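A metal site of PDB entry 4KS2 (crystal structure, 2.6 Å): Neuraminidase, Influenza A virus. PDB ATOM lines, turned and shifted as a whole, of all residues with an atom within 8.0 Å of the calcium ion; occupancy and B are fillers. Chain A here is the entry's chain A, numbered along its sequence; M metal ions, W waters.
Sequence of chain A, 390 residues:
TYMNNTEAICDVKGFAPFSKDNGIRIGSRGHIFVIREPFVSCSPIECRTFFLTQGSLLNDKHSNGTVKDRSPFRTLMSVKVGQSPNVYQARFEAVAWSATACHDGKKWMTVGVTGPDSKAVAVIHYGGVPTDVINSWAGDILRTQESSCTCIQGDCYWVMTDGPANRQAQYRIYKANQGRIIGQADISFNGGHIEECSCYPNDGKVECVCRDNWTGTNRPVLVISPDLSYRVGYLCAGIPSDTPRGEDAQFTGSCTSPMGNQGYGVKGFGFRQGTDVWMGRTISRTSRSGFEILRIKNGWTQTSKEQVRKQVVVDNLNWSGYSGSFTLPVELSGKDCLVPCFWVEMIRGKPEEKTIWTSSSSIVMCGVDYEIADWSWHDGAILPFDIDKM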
ATOM      1  N   HIS A 193      29.130 -10.472  -8.111  1.00  0.00           N
ATOM      2  CA  HIS A 193      29.841 -11.449  -8.925  1.00  0.00           C
ATOM      3  C   HIS A 193      28.863 -12.301  -9.713  1.00  0.00           C
ATOM      4  O   HIS A 193      27.973 -12.938  -9.131  1.00  0.00           O
ATOM      5  CB  HIS A 193      30.735 -12.311  -8.037  1.00  0.00           C
ATOM      6  CG  HIS A 193      31.779 -13.070  -8.789  1.00  0.00           C
ATOM      7  ND1 HIS A 193      33.047 -12.593  -8.982  1.00  0.00           N
ATOM      8  CD2 HIS A 193      31.727 -14.287  -9.400  1.00  0.00           C
ATOM      9  CE1 HIS A 193      33.748 -13.478  -9.674  1.00  0.00           C
ATOM     10  NE2 HIS A 193      32.974 -14.510  -9.939  1.00  0.00           N
ATOM     11  N   CYS A 210      21.756 -15.759 -11.922  1.00  0.00           N
ATOM     12  CA  CYS A 210      23.136 -16.182 -12.138  1.00  0.00           C
ATOM     13  C   CYS A 210      23.803 -16.870 -10.955  1.00  0.00           C
ATOM     14  O   CYS A 210      23.141 -17.322 -10.017  1.00  0.00           O
ATOM     15  CB  CYS A 210      23.953 -14.987 -12.596  1.00  0.00           C
ATOM     16  SG  CYS A 210      23.093 -13.996 -13.812  1.00  0.00           S
ATOM     17  N   ARG A 211      25.122 -16.969 -11.017  1.00  0.00           N
ATOM     18  CA  ARG A 211      25.911 -17.616  -9.980  1.00  0.00           C
ATOM     19  C   ARG A 211      26.961 -16.660  -9.420  1.00  0.00           C
ATOM     20  O   ARG A 211      27.674 -15.983 -10.160  1.00  0.00           O
ATOM     21  CB  ARG A 211      26.589 -18.875 -10.538  1.00  0.00           C
ATOM     22  CG  ARG A 211      27.689 -19.478  -9.684  1.00  0.00           C
ATOM     23  CD  ARG A 211      28.358 -20.641 -10.406  1.00  0.00           C
ATOM     24  NE  ARG A 211      29.444 -21.229  -9.635  1.00  0.00           N
ATOM     25  CZ  ARG A 211      30.136 -22.310  -9.990  1.00  0.00           C
ATOM     26  NH1 ARG A 211      31.104 -22.780  -9.213  1.00  0.00           N
ATOM     27  NH2 ARG A 211      29.862 -22.932 -11.140  1.00  0.00           N
ATOM     28  N   ASP A 212      27.007 -16.588  -8.102  1.00  0.00           N
ATOM     29  CA  ASP A 212      27.996 -15.786  -7.387  1.00  0.00           C
ATOM     30  C   ASP A 212      29.056 -16.759  -6.882  1.00  0.00           C
ATOM     31  O   ASP A 212      28.785 -17.567  -5.987  1.00  0.00           O
ATOM     32  CB  ASP A 212      27.306 -15.092  -6.205  1.00  0.00           C
ATOM     33  CG  ASP A 212      28.176 -14.066  -5.529  1.00  0.00           C
ATOM     34  OD1 ASP A 212      27.705 -12.920  -5.402  1.00  0.00           O
ATOM     35  OD2 ASP A 212      29.304 -14.401  -5.119  1.00  0.00           O
ATOM     36  N   ASN A 213      30.248 -16.695  -7.456  1.00  0.00           N
ATOM     37  CA  ASN A 213      31.299 -17.602  -7.035  1.00  0.00           C
ATOM     38  C   ASN A 213      32.256 -16.947  -6.057  1.00  0.00           C
ATOM     39  O   ASN A 213      33.294 -17.501  -5.714  1.00  0.00           O
ATOM     40  CB  ASN A 213      32.039 -18.163  -8.229  1.00  0.00           C
ATOM     41  CG  ASN A 213      32.526 -19.572  -7.996  1.00  0.00           C
ATOM     42  OD1 ASN A 213      31.748 -20.472  -7.687  1.00  0.00           O
ATOM     43  ND2 ASN A 213      33.828 -19.774  -8.144  1.00  0.00           N
ATOM     44  N   TRP A 214      31.876 -15.761  -5.595  1.00  0.00           N
ATOM     45  CA  TRP A 214      32.713 -14.964  -4.715  1.00  0.00           C
ATOM     46  C   TRP A 214      32.299 -15.130  -3.263  1.00  0.00           C
ATOM     47  O   TRP A 214      32.951 -15.854  -2.516  1.00  0.00           O
ATOM     48  CB  TRP A 214      32.641 -13.493  -5.150  1.00  0.00           C
ATOM     49  CG  TRP A 214      33.608 -12.571  -4.460  1.00  0.00           C
ATOM     50  CD1 TRP A 214      34.547 -12.895  -3.530  1.00  0.00           C
ATOM     51  CD2 TRP A 214      33.709 -11.154  -4.651  1.00  0.00           C
ATOM     52  NE1 TRP A 214      35.233 -11.771  -3.129  1.00  0.00           N
ATOM     53  CE2 TRP A 214      34.729 -10.692  -3.805  1.00  0.00           C
ATOM     54  CE3 TRP A 214      33.033 -10.236  -5.446  1.00  0.00           C
ATOM     55  CZ2 TRP A 214      35.089  -9.355  -3.745  1.00  0.00           C
ATOM     56  CZ3 TRP A 214      33.380  -8.917  -5.375  1.00  0.00           C
ATOM     57  CH2 TRP A 214      34.409  -8.488  -4.539  1.00  0.00           C
ATOM     58  N   THR A 215      31.208 -14.490  -2.857  1.00  0.00           N
ATOM     59  CA  THR A 215      30.754 -14.567  -1.465  1.00  0.00           C
ATOM     60  C   THR A 215      29.259 -14.818  -1.242  1.00  0.00           C
ATOM     61  O   THR A 215      28.839 -15.099  -0.137  1.00  0.00           O
ATOM     62  CB  THR A 215      31.073 -13.281  -0.702  1.00  0.00           C
ATOM     63  OG1 THR A 215      30.375 -12.178  -1.304  1.00  0.00           O
ATOM     64  CG2 THR A 215      32.576 -13.014  -0.700  1.00  0.00           C
ATOM     65  N   GLY A 216      28.446 -14.667  -2.274  1.00  0.00           N
ATOM     66  CA  GLY A 216      27.022 -14.785  -2.086  1.00  0.00           C
ATOM     67  C   GLY A 216      26.523 -16.206  -2.187  1.00  0.00           C
ATOM     68  O   GLY A 216      26.949 -16.970  -3.059  1.00  0.00           O
ATOM     69  N   THR A 217      25.620 -16.585  -1.276  1.00  0.00           N
ATOM     70  CA  THR A 217      24.940 -17.867  -1.390  1.00  0.00           C
ATOM     71  C   THR A 217      23.548 -17.595  -1.929  1.00  0.00           C
ATOM     72  O   THR A 217      22.715 -18.499  -2.029  1.00  0.00           O
ATOM     73  CB  THR A 217      24.852 -18.592  -0.037  1.00  0.00           C
ATOM     74  OG1 THR A 217      24.140 -17.787   0.898  1.00  0.00           O
ATOM     75  CG2 THR A 217      26.236 -18.885   0.504  1.00  0.00           C
ATOM     76  N   ASN A 218      23.312 -16.337  -2.261  1.00  0.00           N
ATOM     77  CA  ASN A 218      22.101 -15.922  -2.967  1.00  0.00           C
ATOM     78  C   ASN A 218      22.479 -15.695  -4.422  1.00  0.00           C
ATOM     79  O   ASN A 218      23.647 -15.450  -4.708  1.00  0.00           O
ATOM     80  CB  ASN A 218      21.518 -14.638  -2.351  1.00  0.00           C
ATOM     81  CG  ASN A 218      22.588 -13.619  -1.988  1.00  0.00           C
ATOM     82  OD1 ASN A 218      23.775 -13.930  -1.966  1.00  0.00           O
ATOM     83  ND2 ASN A 218      22.165 -12.391  -1.681  1.00  0.00           N
ATOM     84  N   ARG A 219      21.519 -15.776  -5.336  1.00  0.00           N
ATOM     85  CA  ARG A 219      21.854 -15.680  -6.765  1.00  0.00           C
ATOM     86  C   ARG A 219      21.644 -14.288  -7.335  1.00  0.00           C
ATOM     87  O   ARG A 219      20.570 -13.712  -7.220  1.00  0.00           O
ATOM     88  CB  ARG A 219      21.084 -16.727  -7.579  1.00  0.00           C
ATOM     89  CG  ARG A 219      21.536 -18.142  -7.293  1.00  0.00           C
ATOM     90  CD  ARG A 219      20.842 -19.162  -8.180  1.00  0.00           C
ATOM     91  NE  ARG A 219      21.226 -20.520  -7.807  1.00  0.00           N
ATOM     92  CZ  ARG A 219      22.357 -21.117  -8.204  1.00  0.00           C
ATOM     93  NH1 ARG A 219      22.618 -22.355  -7.817  1.00  0.00           N
ATOM     94  NH2 ARG A 219      23.210 -20.477  -8.973  1.00  0.00           N
ATOM     95  N   PRO A 220      22.684 -13.748  -7.970  1.00  0.00           N
ATOM     96  CA  PRO A 220      22.505 -12.470  -8.655  1.00  0.00           C
ATOM     97  C   PRO A 220      21.445 -12.547  -9.744  1.00  0.00           C
ATOM     98  O   PRO A 220      21.383 -13.526 -10.480  1.00  0.00           O
ATOM     99  CB  PRO A 220      23.894 -12.186  -9.243  1.00  0.00           C
ATOM    100  CG  PRO A 220      24.681 -13.448  -9.052  1.00  0.00           C
ATOM    101  CD  PRO A 220      24.087 -14.165  -7.914  1.00  0.00           C
ATOM    102  N   SER A 241      19.858 -20.217  -2.754  1.00  0.00           N
ATOM    103  CA  SER A 241      19.733 -21.262  -3.753  1.00  0.00           C
ATOM    104  C   SER A 241      21.049 -21.640  -4.444  1.00  0.00           C
ATOM    105  O   SER A 241      21.031 -22.173  -5.561  1.00  0.00           O
ATOM    106  CB  SER A 241      18.659 -20.891  -4.784  1.00  0.00           C
ATOM    107  OG  SER A 241      19.061 -19.789  -5.565  1.00  0.00           O
ATOM    108  N   ASP A 242      22.167 -21.361  -3.797  1.00  0.00           N
ATOM    109  CA  ASP A 242      23.485 -21.735  -4.310  1.00  0.00           C
ATOM    110  C   ASP A 242      23.969 -22.932  -3.503  1.00  0.00           C
ATOM    111  O   ASP A 242      23.319 -23.342  -2.547  1.00  0.00           O
ATOM    112  CB  ASP A 242      24.449 -20.573  -4.120  1.00  0.00           C
ATOM    113  CG  ASP A 242      25.564 -20.549  -5.162  1.00  0.00           C
ATOM    114  OD1 ASP A 242      26.122 -19.469  -5.388  1.00  0.00           O
ATOM    115  OD2 ASP A 242      25.879 -21.597  -5.749  1.00  0.00           O
ATOM    116  N   THR A 243      25.098 -23.502  -3.885  1.00  0.00           N
ATOM    117  CA  THR A 243      25.720 -24.559  -3.103  1.00  0.00           C
ATOM    118  C   THR A 243      27.219 -24.420  -3.195  1.00  0.00           C
ATOM    119  O   THR A 243      27.765 -24.458  -4.288  1.00  0.00           O
ATOM    120  CB  THR A 243      25.355 -25.933  -3.628  1.00  0.00           C
ATOM    121  OG1 THR A 243      23.941 -26.098  -3.587  1.00  0.00           O
ATOM    122  CG2 THR A 243      26.007 -26.990  -2.782  1.00  0.00           C
ATOM    123  N   PRO A 244      27.913 -24.269  -2.048  1.00  0.00           N
ATOM    124  CA  PRO A 244      27.547 -24.308  -0.630  1.00  0.00           C
ATOM    125  C   PRO A 244      26.744 -23.114  -0.146  1.00  0.00           C
ATOM    126  O   PRO A 244      26.939 -22.008  -0.629  1.00  0.00           O
ATOM    127  CB  PRO A 244      28.910 -24.305   0.083  1.00  0.00           C
ATOM    128  CG  PRO A 244      29.949 -24.466  -0.982  1.00  0.00           C
ATOM    129  CD  PRO A 244      29.334 -23.921  -2.223  1.00  0.00           C
ATOM    130  N   ARG A 245      25.859 -23.355   0.817  1.00  0.00           N
ATOM    131  CA  ARG A 245      25.007 -22.313   1.402  1.00  0.00           C
ATOM    132  C   ARG A 245      24.700 -22.709   2.842  1.00  0.00           C
ATOM    133  O   ARG A 245      24.911 -23.862   3.234  1.00  0.00           O
ATOM    134  CB  ARG A 245      23.706 -22.166   0.608  1.00  0.00           C
ATOM    135  CG  ARG A 245      22.863 -23.428   0.646  1.00  0.00           C
ATOM    136  CD  ARG A 245      21.457 -23.234   0.086  1.00  0.00           C
ATOM    137  NE  ARG A 245      20.661 -24.446   0.266  1.00  0.00           N
ATOM    138  CZ  ARG A 245      20.774 -25.522  -0.496  1.00  0.00           C
ATOM    139  NH1 ARG A 245      20.014 -26.584  -0.271  1.00  0.00           N
ATOM    140  NH2 ARG A 245      21.633 -25.547  -1.501  1.00  0.00           N
ATOM    141  N   MET A 259      24.666 -12.141   0.221  1.00  0.00           N
ATOM    142  CA  MET A 259      24.577 -12.585   1.607  1.00  0.00           C
ATOM    143  C   MET A 259      25.136 -13.988   1.689  1.00  0.00           C
ATOM    144  O   MET A 259      25.121 -14.714   0.702  1.00  0.00           O
ATOM    145  CB  MET A 259      23.126 -12.595   2.054  1.00  0.00           C
ATOM    146  CG  MET A 259      22.471 -11.242   2.040  1.00  0.00           C
ATOM    147  SD  MET A 259      22.799 -10.393   3.580  1.00  0.00           S
ATOM    148  CE  MET A 259      21.782  -8.947   3.371  1.00  0.00           C
ATOM    149  N   ASN A 261      28.416 -15.390   3.254  1.00  0.00           N
ATOM    150  CA  ASN A 261      29.783 -15.602   3.738  1.00  0.00           C
ATOM    151  C   ASN A 261      30.556 -16.803   3.144  1.00  0.00           C
ATOM    152  O   ASN A 261      31.772 -16.743   3.024  1.00  0.00           O
ATOM    153  CB  ASN A 261      29.866 -15.631   5.261  1.00  0.00           C
ATOM    154  CG  ASN A 261      31.283 -15.514   5.780  1.00  0.00           C
ATOM    155  OD1 ASN A 261      32.054 -14.683   5.299  1.00  0.00           O
ATOM    156  ND2 ASN A 261      31.649 -16.363   6.737  1.00  0.00           N
ATOM    157  N   GLN A 262      29.891 -17.890   2.803  1.00  0.00           N
ATOM    158  CA  GLN A 262      30.588 -18.960   2.105  1.00  0.00           C
ATOM    159  C   GLN A 262      30.821 -18.539   0.664  1.00  0.00           C
ATOM    160  O   GLN A 262      30.010 -17.828   0.081  1.00  0.00           O
ATOM    161  CB  GLN A 262      29.810 -20.264   2.191  1.00  0.00           C
ATOM    162  CG  GLN A 262      30.249 -21.209   3.300  1.00  0.00           C
ATOM    163  CD  GLN A 262      31.436 -22.101   2.905  1.00  0.00           C
ATOM    164  OE1 GLN A 262      32.371 -21.651   2.238  1.00  0.00           O
ATOM    165  NE2 GLN A 262      31.391 -23.356   3.327  1.00  0.00           N
ATOM    166  N   GLY A 263      31.934 -18.972   0.077  1.00  0.00           N
ATOM    167  CA  GLY A 263      32.227 -18.670  -1.306  1.00  0.00           C
ATOM    168  C   GLY A 263      31.688 -19.753  -2.230  1.00  0.00           C
ATOM    169  O   GLY A 263      30.555 -20.198  -2.053  1.00  0.00           O
ATOM    170  N   TYR A 264      32.488 -20.137  -3.218  1.00  0.00           N
ATOM    171  CA  TYR A 264      32.153 -21.210  -4.149  1.00  0.00           C
ATOM    172  C   TYR A 264      30.766 -21.067  -4.813  1.00  0.00           C
ATOM    173  O   TYR A 264      30.152 -19.980  -4.771  1.00  0.00           O
ATOM    174  CB  TYR A 264      32.326 -22.567  -3.456  1.00  0.00           C
ATOM    175  CG  TYR A 264      32.481 -23.756  -4.386  1.00  0.00           C
ATOM    176  CD1 TYR A 264      33.199 -23.662  -5.553  1.00  0.00           C
ATOM    177  CD2 TYR A 264      31.916 -24.986  -4.061  1.00  0.00           C
ATOM    178  CE1 TYR A 264      33.341 -24.759  -6.411  1.00  0.00           C
ATOM    179  CE2 TYR A 264      32.044 -26.078  -4.881  1.00  0.00           C
ATOM    180  CZ  TYR A 264      32.769 -25.960  -6.063  1.00  0.00           C
ATOM    181  OH  TYR A 264      32.902 -27.055  -6.891  1.00  0.00           O
ATOM    182  N   GLY A 265      30.262 -22.138  -5.413  1.00  0.00           N
ATOM    183  CA  GLY A 265      28.955 -22.129  -6.038  1.00  0.00           C
ATOM    184  C   GLY A 265      28.685 -23.216  -7.059  1.00  0.00           C
ATOM    185  O   GLY A 265      29.500 -24.124  -7.267  1.00  0.00           O
ATOM    186  N   VAL A 266      27.524 -23.116  -7.702  1.00  0.00           N
ATOM    187  CA  VAL A 266      27.123 -24.003  -8.797  1.00  0.00           C
ATOM    188  C   VAL A 266      26.148 -23.261  -9.682  1.00  0.00           C
ATOM    189  O   VAL A 266      25.391 -22.417  -9.210  1.00  0.00           O
ATOM    190  CB  VAL A 266      26.445 -25.296  -8.266  1.00  0.00           C
ATOM    191  CG1 VAL A 266      25.053 -24.994  -7.737  1.00  0.00           C
ATOM    192  CG2 VAL A 266      26.390 -26.357  -9.364  1.00  0.00           C
HETATM  193 CA    CA M   1      28.197 -18.928  -4.107  1.00  0.00          CA
HETATM  194  O   HOH W   1      28.249 -20.299  -2.399  1.00  0.00           O
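The calcium ion is bound by water W1 (2.2 Å), the backbone carbonyl oxygen (O) of Tyr 264 (2.3 Å), the backbone carbonyl oxygen (O) of Asp 212 (2.4 Å), the side-chain carboxylate (OD1) of Asp 242 (2.5 Å) and the backbone carbonyl oxygen (O) of Gly 216 (2.5 Å).
Merely in contact with the calcium ion: Gly 263 (3.4 Å) and Gly 265 (3.8 Å). Of the 24 residues printed, 6 come within 4 Å of the calcium ion. The nearest printed residue that does not touch the calcium ion is Thr 217 (4.4 Å).
NH1 of Arg 211 sits at hydrogen-bond distance from O of Gly 265, 2.9 Å away. OD2 of Asp 242 is in hydrogen-bond range of N of Val 266. OD2 of Asp 212 is in hydrogen-bond range of N of Thr 215 (3.0 Å). OD2 of Asp 242 lies within salt-bridge range of NH1 of Arg 219 (3.9 Å). OD2 of Asp 212 is in hydrogen-bond range of N of Gly 216, at 3.0 Å. N of Asp 242 sits at hydrogen-bond distance from O of Thr 217, at 3.4 Å. OD1 of Asn 213 is in hydrogen-bond range of N of Gly 265 (3.2 Å). O of Tyr 264 sits close to OD1 of Asn 213 (3.4 Å).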
